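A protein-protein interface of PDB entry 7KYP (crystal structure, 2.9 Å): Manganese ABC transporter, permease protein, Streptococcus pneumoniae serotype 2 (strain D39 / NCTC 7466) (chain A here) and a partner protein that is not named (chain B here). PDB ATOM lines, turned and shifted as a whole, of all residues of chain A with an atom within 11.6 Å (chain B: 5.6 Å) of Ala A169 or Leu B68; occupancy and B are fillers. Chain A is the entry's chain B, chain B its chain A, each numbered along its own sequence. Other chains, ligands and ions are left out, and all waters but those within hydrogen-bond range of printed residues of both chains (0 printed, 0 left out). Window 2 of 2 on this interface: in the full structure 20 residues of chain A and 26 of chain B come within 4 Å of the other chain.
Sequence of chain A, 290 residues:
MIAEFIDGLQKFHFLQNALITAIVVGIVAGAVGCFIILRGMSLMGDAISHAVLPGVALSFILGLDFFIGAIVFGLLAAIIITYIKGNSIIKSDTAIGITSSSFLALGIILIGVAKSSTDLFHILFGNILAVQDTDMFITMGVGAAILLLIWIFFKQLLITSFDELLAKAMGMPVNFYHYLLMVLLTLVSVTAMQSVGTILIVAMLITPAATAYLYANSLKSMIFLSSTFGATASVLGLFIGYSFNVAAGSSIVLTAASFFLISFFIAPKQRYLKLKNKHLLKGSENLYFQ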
ATOM      1  N   ILE A 159      18.817  11.068 -15.026  1.00  0.00           N
ATOM      2  CA  ILE A 159      18.026  10.987 -13.791  1.00  0.00           C
ATOM      3  C   ILE A 159      18.172  12.251 -12.948  1.00  0.00           C
ATOM      4  O   ILE A 159      17.181  12.783 -12.455  1.00  0.00           O
ATOM      5  CB  ILE A 159      18.395   9.752 -12.932  1.00  0.00           C
ATOM      6  CG1 ILE A 159      18.006   8.465 -13.669  1.00  0.00           C
ATOM      7  CG2 ILE A 159      17.685   9.797 -11.579  1.00  0.00           C
ATOM      8  CD1 ILE A 159      18.167   7.197 -12.854  1.00  0.00           C
ATOM      9  N   THR A 160      19.405  12.729 -12.792  1.00  0.00           N
ATOM     10  CA  THR A 160      19.679  13.894 -11.949  1.00  0.00           C
ATOM     11  C   THR A 160      19.022  15.173 -12.478  1.00  0.00           C
ATOM     12  O   THR A 160      18.615  16.031 -11.696  1.00  0.00           O
ATOM     13  CB  THR A 160      21.194  14.130 -11.788  1.00  0.00           C
ATOM     14  OG1 THR A 160      21.813  14.199 -13.078  1.00  0.00           O
ATOM     15  CG2 THR A 160      21.829  13.005 -10.974  1.00  0.00           C
ATOM     16  N   ASP A 163      14.775  13.892 -12.391  1.00  0.00           N
ATOM     17  CA  ASP A 163      14.253  13.581 -11.063  1.00  0.00           C
ATOM     18  C   ASP A 163      15.408  13.436 -10.069  1.00  0.00           C
ATOM     19  O   ASP A 163      15.904  12.335  -9.827  1.00  0.00           O
ATOM     20  CB  ASP A 163      13.413  12.297 -11.131  1.00  0.00           C
ATOM     21  CG  ASP A 163      12.594  12.058  -9.875  1.00  0.00           C
ATOM     22  OD1 ASP A 163      12.965  12.572  -8.799  1.00  0.00           O
ATOM     23  OD2 ASP A 163      11.576  11.341  -9.964  1.00  0.00           O
ATOM     24  N   GLU A 164      15.829  14.562  -9.499  1.00  0.00           N
ATOM     25  CA  GLU A 164      16.934  14.581  -8.541  1.00  0.00           C
ATOM     26  C   GLU A 164      16.545  13.933  -7.210  1.00  0.00           C
ATOM     27  O   GLU A 164      17.401  13.398  -6.505  1.00  0.00           O
ATOM     28  CB  GLU A 164      17.413  16.016  -8.298  1.00  0.00           C
ATOM     29  CG  GLU A 164      18.810  16.105  -7.702  1.00  0.00           C
ATOM     30  CD  GLU A 164      19.181  17.512  -7.278  1.00  0.00           C
ATOM     31  OE1 GLU A 164      18.436  18.109  -6.472  1.00  0.00           O
ATOM     32  OE2 GLU A 164      20.225  18.017  -7.742  1.00  0.00           O
ATOM     33  N   LEU A 165      15.258  13.980  -6.875  1.00  0.00           N
ATOM     34  CA  LEU A 165      14.761  13.393  -5.629  1.00  0.00           C
ATOM     35  C   LEU A 165      14.807  11.861  -5.663  1.00  0.00           C
ATOM     36  O   LEU A 165      14.977  11.220  -4.626  1.00  0.00           O
ATOM     37  CB  LEU A 165      13.337  13.881  -5.337  1.00  0.00           C
ATOM     38  CG  LEU A 165      12.921  13.920  -3.866  1.00  0.00           C
ATOM     39  CD1 LEU A 165      13.681  15.003  -3.114  1.00  0.00           C
ATOM     40  CD2 LEU A 165      11.422  14.149  -3.752  1.00  0.00           C
ATOM     41  N   LEU A 166      14.653  11.283  -6.854  1.00  0.00           N
ATOM     42  CA  LEU A 166      14.813   9.839  -7.040  1.00  0.00           C
ATOM     43  C   LEU A 166      16.289   9.440  -6.971  1.00  0.00           C
ATOM     44  O   LEU A 166      16.621   8.371  -6.452  1.00  0.00           O
ATOM     45  CB  LEU A 166      14.217   9.395  -8.381  1.00  0.00           C
ATOM     46  CG  LEU A 166      14.272   7.893  -8.692  1.00  0.00           C
ATOM     47  CD1 LEU A 166      13.461   7.096  -7.681  1.00  0.00           C
ATOM     48  CD2 LEU A 166      13.781   7.626 -10.106  1.00  0.00           C
ATOM     49  N   ALA A 167      17.162  10.294  -7.502  1.00  0.00           N
ATOM     50  CA  ALA A 167      18.608  10.060  -7.467  1.00  0.00           C
ATOM     51  C   ALA A 167      19.144  10.019  -6.035  1.00  0.00           C
ATOM     52  O   ALA A 167      19.994   9.187  -5.713  1.00  0.00           O
ATOM     53  CB  ALA A 167      19.337  11.127  -8.269  1.00  0.00           C
ATOM     54  N   LYS A 168      18.648  10.918  -5.188  1.00  0.00           N
ATOM     55  CA  LYS A 168      19.032  10.949  -3.775  1.00  0.00           C
ATOM     56  C   LYS A 168      18.532   9.723  -3.013  1.00  0.00           C
ATOM     57  O   LYS A 168      19.203   9.244  -2.098  1.00  0.00           O
ATOM     58  CB  LYS A 168      18.518  12.225  -3.103  1.00  0.00           C
ATOM     59  CG  LYS A 168      19.229  13.490  -3.554  1.00  0.00           C
ATOM     60  CD  LYS A 168      18.667  14.718  -2.858  1.00  0.00           C
ATOM     61  CE  LYS A 168      19.385  15.983  -3.295  1.00  0.00           C
ATOM     62  NZ  LYS A 168      18.759  17.205  -2.716  1.00  0.00           N
ATOM     63  N   ALA A 169      17.359   9.218  -3.391  1.00  0.00           N
ATOM     64  CA  ALA A 169      16.796   8.010  -2.781  1.00  0.00           C
ATOM     65  C   ALA A 169      17.573   6.746  -3.160  1.00  0.00           C
ATOM     66  O   ALA A 169      17.554   5.760  -2.422  1.00  0.00           O
ATOM     67  CB  ALA A 169      15.332   7.859  -3.166  1.00  0.00           C
ATOM     68  N   MET A 170      18.243   6.778  -4.312  1.00  0.00           N
ATOM     69  CA  MET A 170      19.080   5.665  -4.770  1.00  0.00           C
ATOM     70  C   MET A 170      20.526   5.769  -4.273  1.00  0.00           C
ATOM     71  O   MET A 170      21.324   4.854  -4.488  1.00  0.00           O
ATOM     72  CB  MET A 170      19.069   5.597  -6.300  1.00  0.00           C
ATOM     73  CG  MET A 170      17.718   5.231  -6.890  1.00  0.00           C
ATOM     74  SD  MET A 170      17.606   5.618  -8.645  1.00  0.00           S
ATOM     75  CE  MET A 170      16.108   4.743  -9.090  1.00  0.00           C
ATOM     76  N   GLY A 171      20.862   6.882  -3.623  1.00  0.00           N
ATOM     77  CA  GLY A 171      22.194   7.087  -3.060  1.00  0.00           C
ATOM     78  C   GLY A 171      23.216   7.614  -4.051  1.00  0.00           C
ATOM     79  O   GLY A 171      24.419   7.443  -3.850  1.00  0.00           O
ATOM     80  N   MET A 172      22.749   8.262  -5.116  1.00  0.00           N
ATOM     81  CA  MET A 172      23.645   8.828  -6.121  1.00  0.00           C
ATOM     82  C   MET A 172      24.237  10.141  -5.617  1.00  0.00           C
ATOM     83  O   MET A 172      23.541  10.920  -4.962  1.00  0.00           O
ATOM     84  CB  MET A 172      22.899   9.080  -7.434  1.00  0.00           C
ATOM     85  CG  MET A 172      22.378   7.823  -8.112  1.00  0.00           C
ATOM     86  SD  MET A 172      21.417   8.183  -9.595  1.00  0.00           S
ATOM     87  CE  MET A 172      22.663   8.920 -10.649  1.00  0.00           C
ATOM     88  N   PRO A 173      25.523  10.395  -5.920  1.00  0.00           N
ATOM     89  CA  PRO A 173      26.130  11.675  -5.565  1.00  0.00           C
ATOM     90  C   PRO A 173      25.684  12.781  -6.525  1.00  0.00           C
ATOM     91  O   PRO A 173      26.320  13.010  -7.554  1.00  0.00           O
ATOM     92  CB  PRO A 173      27.631  11.394  -5.685  1.00  0.00           C
ATOM     93  CG  PRO A 173      27.729  10.330  -6.723  1.00  0.00           C
ATOM     94  CD  PRO A 173      26.478   9.502  -6.605  1.00  0.00           C
ATOM     95  N   VAL A 174      24.584  13.447  -6.183  1.00  0.00           N
ATOM     96  CA  VAL A 174      24.011  14.491  -7.040  1.00  0.00           C
ATOM     97  C   VAL A 174      24.917  15.723  -7.160  1.00  0.00           C
ATOM     98  O   VAL A 174      24.884  16.423  -8.173  1.00  0.00           O
ATOM     99  CB  VAL A 174      22.606  14.936  -6.564  1.00  0.00           C
ATOM    100  CG1 VAL A 174      21.654  13.747  -6.512  1.00  0.00           C
ATOM    101  CG2 VAL A 174      22.676  15.651  -5.217  1.00  0.00           C
ATOM    102  N   ASN A 175      25.718  15.977  -6.126  1.00  0.00           N
ATOM    103  CA  ASN A 175      26.662  17.096  -6.134  1.00  0.00           C
ATOM    104  C   ASN A 175      27.795  16.877  -7.139  1.00  0.00           C
ATOM    105  O   ASN A 175      28.276  17.832  -7.748  1.00  0.00           O
ATOM    106  CB  ASN A 175      27.246  17.318  -4.732  1.00  0.00           C
ATOM    107  CG  ASN A 175      26.192  17.713  -3.710  1.00  0.00           C
ATOM    108  OD1 ASN A 175      25.140  18.257  -4.055  1.00  0.00           O
ATOM    109  ND2 ASN A 175      26.473  17.443  -2.440  1.00  0.00           N
ATOM    110  N   LEU B  48      14.702   8.092   4.608  1.00  0.00           N
ATOM    111  CA  LEU B  48      15.627   7.750   3.524  1.00  0.00           C
ATOM    112  C   LEU B  48      16.964   8.487   3.625  1.00  0.00           C
ATOM    113  O   LEU B  48      17.987   7.984   3.156  1.00  0.00           O
ATOM    114  CB  LEU B  48      14.985   8.048   2.165  1.00  0.00           C
ATOM    115  CG  LEU B  48      13.794   7.163   1.789  1.00  0.00           C
ATOM    116  CD1 LEU B  48      12.986   7.787   0.662  1.00  0.00           C
ATOM    117  CD2 LEU B  48      14.257   5.765   1.407  1.00  0.00           C
ATOM    118  N   ILE B  50      17.224  11.833   2.558  1.00  0.00           N
ATOM    119  CA  ILE B  50      17.243  12.775   1.440  1.00  0.00           C
ATOM    120  C   ILE B  50      17.456  14.202   1.953  1.00  0.00           C
ATOM    121  O   ILE B  50      17.989  15.052   1.236  1.00  0.00           O
ATOM    122  CB  ILE B  50      15.937  12.693   0.614  1.00  0.00           C
ATOM    123  CG1 ILE B  50      15.775  11.291   0.012  1.00  0.00           C
ATOM    124  CG2 ILE B  50      15.929  13.739  -0.496  1.00  0.00           C
ATOM    125  CD1 ILE B  50      14.392  11.006  -0.536  1.00  0.00           C
ATOM    126  N   VAL B  64      19.607   2.183   7.036  1.00  0.00           N
ATOM    127  CA  VAL B  64      18.861   2.617   5.848  1.00  0.00           C
ATOM    128  C   VAL B  64      19.781   3.236   4.797  1.00  0.00           C
ATOM    129  O   VAL B  64      19.727   2.867   3.622  1.00  0.00           O
ATOM    130  CB  VAL B  64      17.759   3.643   6.215  1.00  0.00           C
ATOM    131  CG1 VAL B  64      17.181   4.311   4.970  1.00  0.00           C
ATOM    132  CG2 VAL B  64      16.651   2.977   7.017  1.00  0.00           C
ATOM    133  N   LYS B  65      20.615   4.177   5.228  1.00  0.00           N
ATOM    134  CA  LYS B  65      21.515   4.904   4.327  1.00  0.00           C
ATOM    135  C   LYS B  65      22.533   3.999   3.628  1.00  0.00           C
ATOM    136  O   LYS B  65      22.985   4.313   2.525  1.00  0.00           O
ATOM    137  CB  LYS B  65      22.234   6.022   5.092  1.00  0.00           C
ATOM    138  CG  LYS B  65      21.320   7.176   5.485  1.00  0.00           C
ATOM    139  CD  LYS B  65      21.678   7.764   6.843  1.00  0.00           C
ATOM    140  CE  LYS B  65      21.152   6.900   7.980  1.00  0.00           C
ATOM    141  NZ  LYS B  65      21.398   7.510   9.316  1.00  0.00           N
ATOM    142  N   LYS B  66      22.885   2.881   4.265  1.00  0.00           N
ATOM    143  CA  LYS B  66      23.802   1.900   3.678  1.00  0.00           C
ATOM    144  C   LYS B  66      23.078   0.725   3.006  1.00  0.00           C
ATOM    145  O   LYS B  66      23.693  -0.310   2.739  1.00  0.00           O
ATOM    146  CB  LYS B  66      24.752   1.368   4.755  1.00  0.00           C
ATOM    147  N   SER B  67      21.782   0.882   2.734  1.00  0.00           N
ATOM    148  CA  SER B  67      20.987  -0.156   2.072  1.00  0.00           C
ATOM    149  C   SER B  67      19.839   0.469   1.278  1.00  0.00           C
ATOM    150  O   SER B  67      18.681   0.066   1.410  1.00  0.00           O
ATOM    151  CB  SER B  67      20.444  -1.155   3.099  1.00  0.00           C
ATOM    152  OG  SER B  67      21.497  -1.853   3.741  1.00  0.00           O
ATOM    153  N   LEU B  68      20.177   1.456   0.451  1.00  0.00           N
ATOM    154  CA  LEU B  68      19.192   2.166  -0.366  1.00  0.00           C
ATOM    155  C   LEU B  68      18.726   1.330  -1.559  1.00  0.00           C
ATOM    156  O   LEU B  68      17.622   1.533  -2.066  1.00  0.00           O
ATOM    157  CB  LEU B  68      19.766   3.500  -0.853  1.00  0.00           C
ATOM    158  CG  LEU B  68      20.079   4.526   0.241  1.00  0.00           C
ATOM    159  CD1 LEU B  68      20.934   5.658  -0.308  1.00  0.00           C
ATOM    160  CD2 LEU B  68      18.801   5.071   0.864  1.00  0.00           C
ATOM    161  N   HIS B  69      19.569   0.398  -2.003  1.00  0.00           N
ATOM    162  CA  HIS B  69      19.212  -0.530  -3.085  1.00  0.00           C
ATOM    163  C   HIS B  69      17.997  -1.409  -2.756  1.00  0.00           C
ATOM    164  O   HIS B  69      17.282  -1.845  -3.660  1.00  0.00           O
ATOM    165  CB  HIS B  69      20.412  -1.409  -3.469  1.00  0.00           C
ATOM    166  CG  HIS B  69      20.912  -2.283  -2.357  1.00  0.00           C
ATOM    167  ND1 HIS B  69      21.901  -1.885  -1.484  1.00  0.00           N
ATOM    168  CD2 HIS B  69      20.566  -3.539  -1.986  1.00  0.00           C
ATOM    169  CE1 HIS B  69      22.138  -2.854  -0.619  1.00  0.00           C
ATOM    170  NE2 HIS B  69      21.342  -3.870  -0.902  1.00  0.00           N
ATOM    171  N   ARG B  70      17.770  -1.662  -1.467  1.00  0.00           N
ATOM    172  CA  ARG B  70      16.610  -2.434  -1.012  1.00  0.00           C
ATOM    173  C   ARG B  70      15.307  -1.628  -0.970  1.00  0.00           C
ATOM    174  O   ARG B  70      14.227  -2.214  -0.873  1.00  0.00           O
ATOM    175  CB  ARG B  70      16.873  -3.016   0.379  1.00  0.00           C
ATOM    176  CG  ARG B  70      18.001  -4.034   0.435  1.00  0.00           C
ATOM    177  CD  ARG B  70      18.061  -4.701   1.799  1.00  0.00           C
ATOM    178  NE  ARG B  70      16.841  -5.455   2.086  1.00  0.00           N
ATOM    179  CZ  ARG B  70      16.505  -5.938   3.281  1.00  0.00           C
ATOM    180  NH1 ARG B  70      17.292  -5.758   4.338  1.00  0.00           N
ATOM    181  NH2 ARG B  70      15.366  -6.608   3.423  1.00  0.00           N
ATOM    182  N   ILE B  71      15.406  -0.300  -1.021  1.00  0.00           N
ATOM    183  CA  ILE B  71      14.239   0.584  -0.944  1.00  0.00           C
ATOM    184  C   ILE B  71      13.908   1.168  -2.316  1.00  0.00           C
ATOM    185  O   ILE B  71      14.784   1.303  -3.172  1.00  0.00           O
ATOM    186  CB  ILE B  71      14.477   1.760   0.034  1.00  0.00           C
ATOM    187  CG1 ILE B  71      15.075   1.267   1.355  1.00  0.00           C
ATOM    188  CG2 ILE B  71      13.179   2.514   0.301  1.00  0.00           C
ATOM    189  CD1 ILE B  71      15.600   2.378   2.240  1.00  0.00           C
ATOM    190  N   ALA B  72      12.634   1.498  -2.513  1.00  0.00           N
ATOM    191  CA  ALA B  72      12.177   2.227  -3.692  1.00  0.00           C
ATOM    192  C   ALA B  72      11.277   3.378  -3.248  1.00  0.00           C
ATOM    193  O   ALA B  72      10.354   3.181  -2.456  1.00  0.00           O
ATOM    194  CB  ALA B  72      11.427   1.299  -4.633  1.00  0.00           C
ATOM    195  N   TYR B  73      11.558   4.575  -3.762  1.00  0.00           N
ATOM    196  CA  TYR B  73      10.830   5.784  -3.386  1.00  0.00           C
ATOM    197  C   TYR B  73      10.029   6.312  -4.573  1.00  0.00           C
ATOM    198  O   TYR B  73      10.566   6.473  -5.672  1.00  0.00           O
ATOM    199  CB  TYR B  73      11.814   6.849  -2.897  1.00  0.00           C
ATOM    200  CG  TYR B  73      11.169   8.114  -2.369  1.00  0.00           C
ATOM    201  CD1 TYR B  73      10.255   8.067  -1.319  1.00  0.00           C
ATOM    202  CD2 TYR B  73      11.489   9.359  -2.903  1.00  0.00           C
ATOM    203  CE1 TYR B  73       9.670   9.223  -0.826  1.00  0.00           C
ATOM    204  CE2 TYR B  73      10.909  10.520  -2.416  1.00  0.00           C
ATOM    205  CZ  TYR B  73      10.000  10.447  -1.377  1.00  0.00           C
ATOM    206  OH  TYR B  73       9.422  11.597  -0.889  1.00  0.00           O
ATOM    207  N   GLN B 150      12.779  -1.833  -9.847  1.00  0.00           N
ATOM    208  CA  GLN B 150      13.820  -1.827  -8.815  1.00  0.00           C
ATOM    209  C   GLN B 150      13.867  -3.140  -8.031  1.00  0.00           C
ATOM    210  O   GLN B 150      14.918  -3.507  -7.503  1.00  0.00           O
ATOM    211  CB  GLN B 150      13.613  -0.670  -7.833  1.00  0.00           C
ATOM    212  CG  GLN B 150      13.752   0.713  -8.450  1.00  0.00           C
ATOM    213  CD  GLN B 150      13.890   1.821  -7.417  1.00  0.00           C
ATOM    214  OE1 GLN B 150      14.302   1.586  -6.281  1.00  0.00           O
ATOM    215  NE2 GLN B 150      13.553   3.042  -7.816  1.00  0.00           N
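The side-chain carboxylate (OE1) of Glu A164 lies within salt-bridge range of the side-chain amino group (NZ) of Lys A168 (3.9 Å). N of Leu A166 sits at hydrogen-bond distance from OD1 of Asp A163 (2.9 Å). OD1 of Asp A163 lies close to N of Leu A165, 3.3 Å away. O of Ile B71 sits close to OE1 of Gln B150, 3.2 Å away.
Ile B50 touches Leu A165. Leu A165 touches Tyr B73. Leu A166 touches Tyr B73. Lys A168 touches Ile B50 (CD to CG2, 3.7 Å). O of Ala A169 touches CB of Leu B68, at 3.5 Å. Ala A169 touches Tyr B73 (CB to CB, 3.7 Å). Met A170 touches Leu B68 (C to CD1, 3.99 Å). Gln B150 touches Met A170. Gly A171 touches Leu B68 (CA to CD1, 3.3 Å).
Ile A159 touches none of the printed residues of chain B. Thr A160 touches none of the printed residues of chain B. Printed residues of chain B within 4 Å of Leu A166: Tyr B73 (3.6 Å). Of the printed residues of chain B, Lys A168 touches Ile B50 (3.7 Å). Printed residues of chain B within 4 Å of Met A170: Leu B68 and Gln B150. Of chain A, only Leu A165 and Lys A168 come within 4 Å of Ile B50. No residue of chain A comes within 4 Å of Val B64. No residue of chain A comes within 4 Å of Ser B67. Of the printed residues of chain A, Leu B68 touches Ala A169, Met A170 and Gly A171. No residue of chain A comes within 4 Å of Ile B71. Ala B72 touches none of the printed residues of chain A. Tyr B73 touches three residues of chain A. The nearest residue of chain B that does not touch Ala A169 is Ile B50 (4.2 Å). The nearest printed residue of chain B that does not touch Gly A171 is Lys B65 (6.3 Å).
Of the 15 printed residues of chain A, 6 touch a printed residue of chain B. Printed residues of chain A that touch a printed residue of chain B: Leu A165, Leu A166, Lys A168, Ala A169, Met A170 and Gly A171. Hydrophobic or aromatic side chains of chain A that line the printed part of chain B: Leu A165, Leu A166, Ala A169 and Met A170. Hydrophobic or aromatic side chains of chain B within 4 Å of the printed part of chain A: Ile B50, Leu B68 and Tyr B73. Among the printed residues, no Asp or Glu carboxylate lies within 4 Å of a Lys or Arg side-chain nitrogen of the other chain.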
